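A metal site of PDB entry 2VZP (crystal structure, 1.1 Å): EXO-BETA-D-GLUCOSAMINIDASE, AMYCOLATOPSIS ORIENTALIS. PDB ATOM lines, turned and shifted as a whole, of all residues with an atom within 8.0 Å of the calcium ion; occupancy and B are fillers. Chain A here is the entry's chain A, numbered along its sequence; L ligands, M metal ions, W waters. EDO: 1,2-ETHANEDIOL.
OD1 of Asn 32 sits close to OD1 of Asn 121 (3.3 Å). OE1 of Glu 19 is in hydrogen-bond range of ND2 of Asn 32, 2.8 Å away. N of Asn 32 sits at hydrogen-bond distance from O of Ala 17, at 2.9 Å. NH1 of Arg 67 lies within hydrogen-bond range of O of Gly 119 (3.1 Å).
Residues that only touch the calcium ion: Arg 67 (3.9 Å). Four residues have an atom within 4 Å of the calcium ion: Asn 32, Tyr 33, Asn 35 and Arg 67. Along chain A the residues within 4 Å of the calcium ion span positions 32 to 67. The nearest printed residue that does not touch the calcium ion is Asp 34 (4.3 Å).
The calcium ion is bound by O of Tyr 33 (2.3 Å), OD1 of Asn 32 (2.4 Å), water W2 (2.4 Å), OD1 of Asn 35 (2.4 Å), water W1 (2.6 Å), water W3 (2.7 Å) and O2 of the ligand (2.7 Å). The calcium ion has seven donor atoms within binding distance.
Water W2 lies within hydrogen-bond range of O of Asn 117 (2.8 Å), O of Gly 119 (2.9 Å) and NH1 of Arg 67 (3.2 Å).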
ATOM      1  N   GLN A  15     -15.626  19.472 -12.148  1.00  0.00           N
ATOM      2  CA  GLN A  15     -14.491  18.571 -12.419  1.00  0.00           C
ATOM      3  C   GLN A  15     -14.228  18.470 -13.916  1.00  0.00           C
ATOM      4  O   GLN A  15     -14.245  17.389 -14.514  1.00  0.00           O
ATOM      5  CB  GLN A  15     -14.635  17.210 -11.789  1.00  0.00           C
ATOM      6  CG  GLN A  15     -14.790  17.252 -10.262  1.00  0.00           C
ATOM      7  CD  GLN A  15     -14.536  15.916  -9.662  1.00  0.00           C
ATOM      8  OE1 GLN A  15     -13.372  15.507  -9.573  1.00  0.00           O
ATOM      9  NE2 GLN A  15     -15.581  15.172  -9.291  1.00  0.00           N
ATOM     10  N   GLY A  16     -13.966  19.602 -14.539  1.00  0.00           N
ATOM     11  CA  GLY A  16     -13.605  19.659 -15.943  1.00  0.00           C
ATOM     12  C   GLY A  16     -12.846  20.924 -16.242  1.00  0.00           C
ATOM     13  O   GLY A  16     -12.666  21.768 -15.336  1.00  0.00           O
ATOM     14  N   ALA A  17     -12.409  21.093 -17.483  1.00  0.00           N
ATOM     15  CA  ALA A  17     -11.580  22.220 -17.876  1.00  0.00           C
ATOM     16  C   ALA A  17     -11.959  22.675 -19.262  1.00  0.00           C
ATOM     17  O   ALA A  17     -12.229  21.838 -20.140  1.00  0.00           O
ATOM     18  CB  ALA A  17     -10.100  21.826 -17.886  1.00  0.00           C
ATOM     19  N   GLU A  19     -10.817  23.938 -22.681  1.00  0.00           N
ATOM     20  CA  GLU A  19      -9.646  23.793 -23.488  1.00  0.00           C
ATOM     21  C   GLU A  19      -9.946  24.112 -24.939  1.00  0.00           C
ATOM     22  O   GLU A  19     -11.089  24.260 -25.368  1.00  0.00           O
ATOM     23  CB  GLU A  19      -9.002  22.400 -23.304  1.00  0.00           C
ATOM     24  CG  GLU A  19      -8.557  22.231 -21.848  1.00  0.00           C
ATOM     25  CD  GLU A  19      -7.986  20.941 -21.423  1.00  0.00           C
ATOM     26  OE1 GLU A  19      -8.063  19.960 -22.171  1.00  0.00           O
ATOM     27  OE2 GLU A  19      -7.428  20.869 -20.287  1.00  0.00           O
ATOM     28  N   VAL A  31     -15.168  21.509 -23.477  1.00  0.00           N
ATOM     29  CA  VAL A  31     -14.900  21.024 -22.150  1.00  0.00           C
ATOM     30  C   VAL A  31     -14.256  19.659 -22.229  1.00  0.00           C
ATOM     31  O   VAL A  31     -14.769  18.721 -22.872  1.00  0.00           O
ATOM     32  CB  VAL A  31     -16.171  20.976 -21.288  1.00  0.00           C
ATOM     33  CG1 VAL A  31     -15.887  20.304 -19.942  1.00  0.00           C
ATOM     34  CG2 VAL A  31     -16.690  22.403 -21.113  1.00  0.00           C
ATOM     35  N   ASN A  32     -13.131  19.520 -21.543  1.00  0.00           N
ATOM     36  CA  ASN A  32     -12.450  18.281 -21.310  1.00  0.00           C
ATOM     37  C   ASN A  32     -12.843  17.849 -19.891  1.00  0.00           C
ATOM     38  O   ASN A  32     -12.441  18.480 -18.883  1.00  0.00           O
ATOM     39  CB  ASN A  32     -10.937  18.510 -21.423  1.00  0.00           C
ATOM     40  CG  ASN A  32     -10.137  17.252 -21.144  1.00  0.00           C
ATOM     41  OD1 ASN A  32     -10.696  16.243 -20.775  1.00  0.00           O
ATOM     42  ND2 ASN A  32      -8.825  17.359 -21.296  1.00  0.00           N
ATOM     43  N   TYR A  33     -13.733  16.859 -19.775  1.00  0.00           N
ATOM     44  CA  TYR A  33     -14.112  16.344 -18.452  1.00  0.00           C
ATOM     45  C   TYR A  33     -12.876  15.805 -17.765  1.00  0.00           C
ATOM     46  O   TYR A  33     -12.090  15.102 -18.380  1.00  0.00           O
ATOM     47  CB  TYR A  33     -15.100  15.170 -18.617  1.00  0.00           C
ATOM     48  CG  TYR A  33     -16.545  15.488 -18.901  1.00  0.00           C
ATOM     49  CD1 TYR A  33     -16.943  16.222 -20.044  1.00  0.00           C
ATOM     50  CD2 TYR A  33     -17.544  15.008 -18.055  1.00  0.00           C
ATOM     51  CE1 TYR A  33     -18.288  16.453 -20.284  1.00  0.00           C
ATOM     52  CE2 TYR A  33     -18.873  15.240 -18.321  1.00  0.00           C
ATOM     53  CZ  TYR A  33     -19.255  15.949 -19.448  1.00  0.00           C
ATOM     54  OH  TYR A  33     -20.573  16.218 -19.729  1.00  0.00           O
ATOM     55  N   ASP A  34     -12.758  16.013 -16.463  1.00  0.00           N
ATOM     56  CA  ASP A  34     -11.679  15.314 -15.734  1.00  0.00           C
ATOM     57  C   ASP A  34     -11.948  13.811 -15.785  1.00  0.00           C
ATOM     58  O   ASP A  34     -13.107  13.328 -15.895  1.00  0.00           O
ATOM     59  CB  ASP A  34     -11.563  15.781 -14.288  1.00  0.00           C
ATOM     60  CG  ASP A  34     -11.159  17.235 -14.132  1.00  0.00           C
ATOM     61  OD1 ASP A  34     -10.685  17.870 -15.097  1.00  0.00           O
ATOM     62  OD2 ASP A  34     -11.296  17.748 -12.984  1.00  0.00           O
ATOM     63  N   ASN A  35     -10.881  13.041 -15.691  1.00  0.00           N
ATOM     64  CA  ASN A  35     -10.961  11.605 -15.813  1.00  0.00           C
ATOM     65  C   ASN A  35     -11.289  10.990 -14.443  1.00  0.00           C
ATOM     66  O   ASN A  35     -10.456  10.382 -13.753  1.00  0.00           O
ATOM     67  CB  ASN A  35      -9.693  11.023 -16.467  1.00  0.00           C
ATOM     68  CG  ASN A  35      -9.628  11.319 -17.991  1.00  0.00           C
ATOM     69  OD1 ASN A  35      -9.940  12.417 -18.443  1.00  0.00           O
ATOM     70  ND2 ASN A  35      -9.175  10.364 -18.780  1.00  0.00           N
ATOM     71  N   VAL A  36     -12.524  11.210 -14.057  1.00  0.00           N
ATOM     72  CA  VAL A  36     -13.155  10.736 -12.834  1.00  0.00           C
ATOM     73  C   VAL A  36     -14.621  10.523 -13.104  1.00  0.00           C
ATOM     74  O   VAL A  36     -15.221  11.227 -13.941  1.00  0.00           O
ATOM     75  CB  VAL A  36     -13.043  11.720 -11.646  1.00  0.00           C
ATOM     76  CG1 VAL A  36     -11.587  11.922 -11.248  1.00  0.00           C
ATOM     77  CG2 VAL A  36     -13.660  13.054 -11.953  1.00  0.00           C
ATOM     78  N   SER A  39     -17.676  13.810 -13.037  1.00  0.00           N
ATOM     79  CA  SER A  39     -17.439  15.022 -13.779  1.00  0.00           C
ATOM     80  C   SER A  39     -18.689  15.341 -14.606  1.00  0.00           C
ATOM     81  O   SER A  39     -19.403  14.423 -15.049  1.00  0.00           O
ATOM     82  CB  SER A  39     -16.192  14.875 -14.631  1.00  0.00           C
ATOM     83  OG  SER A  39     -16.197  13.656 -15.325  1.00  0.00           O
ATOM     84  N   ARG A  67     -17.097   6.473 -23.192  1.00  0.00           N
ATOM     85  CA  ARG A  67     -17.205   7.315 -22.006  1.00  0.00           C
ATOM     86  C   ARG A  67     -18.644   7.691 -21.768  1.00  0.00           C
ATOM     87  O   ARG A  67     -19.096   8.757 -22.228  1.00  0.00           O
ATOM     88  CB  ARG A  67     -16.344   8.519 -22.221  1.00  0.00           C
ATOM     89  CG  ARG A  67     -14.805   8.148 -22.218  1.00  0.00           C
ATOM     90  CD  ARG A  67     -13.981   9.347 -22.254  1.00  0.00           C
ATOM     91  NE  ARG A  67     -12.559   8.999 -22.256  1.00  0.00           N
ATOM     92  CZ  ARG A  67     -11.669   9.944 -22.309  1.00  0.00           C
ATOM     93  NH1 ARG A  67     -12.059  11.202 -22.361  1.00  0.00           N
ATOM     94  NH2 ARG A  67     -10.396   9.575 -22.327  1.00  0.00           N
ATOM     95  N   TRP A  90      -9.152  13.118 -31.640  1.00  0.00           N
ATOM     96  CA  TRP A  90      -9.753  14.170 -30.805  1.00  0.00           C
ATOM     97  C   TRP A  90     -10.384  15.310 -31.618  1.00  0.00           C
ATOM     98  O   TRP A  90     -11.380  15.892 -31.145  1.00  0.00           O
ATOM     99  CB  TRP A  90      -8.764  14.672 -29.771  1.00  0.00           C
ATOM    100  CG  TRP A  90      -8.444  13.651 -28.735  1.00  0.00           C
ATOM    101  CD1 TRP A  90      -7.282  12.950 -28.578  1.00  0.00           C
ATOM    102  CD2 TRP A  90      -9.295  13.220 -27.664  1.00  0.00           C
ATOM    103  NE1 TRP A  90      -7.361  12.109 -27.513  1.00  0.00           N
ATOM    104  CE2 TRP A  90      -8.584  12.243 -26.931  1.00  0.00           C
ATOM    105  CE3 TRP A  90     -10.593  13.542 -27.260  1.00  0.00           C
ATOM    106  CZ2 TRP A  90      -9.137  11.605 -25.814  1.00  0.00           C
ATOM    107  CZ3 TRP A  90     -11.127  12.928 -26.150  1.00  0.00           C
ATOM    108  CH2 TRP A  90     -10.399  11.931 -25.442  1.00  0.00           C
ATOM    109  N   ALA A 116     -14.893   5.986 -14.390  1.00  0.00           N
ATOM    110  CA  ALA A 116     -13.636   6.586 -14.019  1.00  0.00           C
ATOM    111  C   ALA A 116     -12.879   7.261 -15.148  1.00  0.00           C
ATOM    112  O   ALA A 116     -11.976   8.043 -14.929  1.00  0.00           O
ATOM    113  CB  ALA A 116     -12.721   5.552 -13.275  1.00  0.00           C
ATOM    114  N   ASN A 117     -13.243   6.941 -16.392  1.00  0.00           N
ATOM    115  CA  ASN A 117     -12.728   7.537 -17.611  1.00  0.00           C
ATOM    116  C   ASN A 117     -13.195   9.015 -17.778  1.00  0.00           C
ATOM    117  O   ASN A 117     -12.683   9.724 -18.652  1.00  0.00           O
ATOM    118  CB  ASN A 117     -13.206   6.651 -18.800  1.00  0.00           C
ATOM    119  CG  ASN A 117     -12.877   5.144 -18.599  1.00  0.00           C
ATOM    120  OD1 ASN A 117     -11.706   4.791 -18.565  1.00  0.00           O
ATOM    121  ND2 ASN A 117     -13.901   4.283 -18.475  1.00  0.00           N
ATOM    122  N   GLY A 118     -14.208   9.414 -17.035  1.00  0.00           N
ATOM    123  CA  GLY A 118     -14.837  10.711 -17.253  1.00  0.00           C
ATOM    124  C   GLY A 118     -15.662  10.706 -18.524  1.00  0.00           C
ATOM    125  O   GLY A 118     -16.102   9.674 -19.021  1.00  0.00           O
ATOM    126  N   GLY A 119     -15.939  11.906 -19.010  1.00  0.00           N
ATOM    127  CA  GLY A 119     -16.734  12.096 -20.198  1.00  0.00           C
ATOM    128  C   GLY A 119     -15.920  12.212 -21.463  1.00  0.00           C
ATOM    129  O   GLY A 119     -14.699  12.413 -21.421  1.00  0.00           O
ATOM    130  N   PRO A 120     -16.586  12.137 -22.636  1.00  0.00           N
ATOM    131  CA  PRO A 120     -15.905  12.548 -23.863  1.00  0.00           C
ATOM    132  C   PRO A 120     -15.597  14.063 -23.772  1.00  0.00           C
ATOM    133  O   PRO A 120     -16.170  14.749 -22.920  1.00  0.00           O
ATOM    134  CB  PRO A 120     -16.953  12.270 -24.924  1.00  0.00           C
ATOM    135  CG  PRO A 120     -18.266  12.553 -24.220  1.00  0.00           C
ATOM    136  CD  PRO A 120     -18.037  12.064 -22.797  1.00  0.00           C
ATOM    137  N   ASN A 121     -14.732  14.579 -24.660  1.00  0.00           N
ATOM    138  CA  ASN A 121     -14.702  16.021 -24.784  1.00  0.00           C
ATOM    139  C   ASN A 121     -16.023  16.477 -25.371  1.00  0.00           C
ATOM    140  O   ASN A 121     -16.540  15.846 -26.310  1.00  0.00           O
ATOM    141  CB  ASN A 121     -13.526  16.483 -25.654  1.00  0.00           C
ATOM    142  CG  ASN A 121     -12.195  16.257 -25.022  1.00  0.00           C
ATOM    143  OD1 ASN A 121     -12.058  15.978 -23.823  1.00  0.00           O
ATOM    144  ND2 ASN A 121     -11.142  16.431 -25.817  1.00  0.00           N
HETATM  145  C1  EDO L   1      -8.455  12.540 -22.016  1.00  0.00           C
HETATM  146  O1  EDO L   1      -8.445  11.139 -22.188  1.00  0.00           O
HETATM  147  C2  EDO L   1      -9.818  13.082 -21.615  1.00  0.00           C
HETATM  148  O2  EDO L   1     -10.477  13.810 -22.676  1.00  0.00           O
HETATM  149 CA    CA M   1     -10.929  14.040 -19.989  1.00  0.00          CA
HETATM  150  O   HOH W   1      -9.096  15.247 -18.602  1.00  0.00           O
HETATM  151  O   HOH W   2     -12.561  12.386 -19.483  1.00  0.00           O
HETATM  152  O   HOH W   3     -12.953  14.592 -21.634  1.00  0.00           O
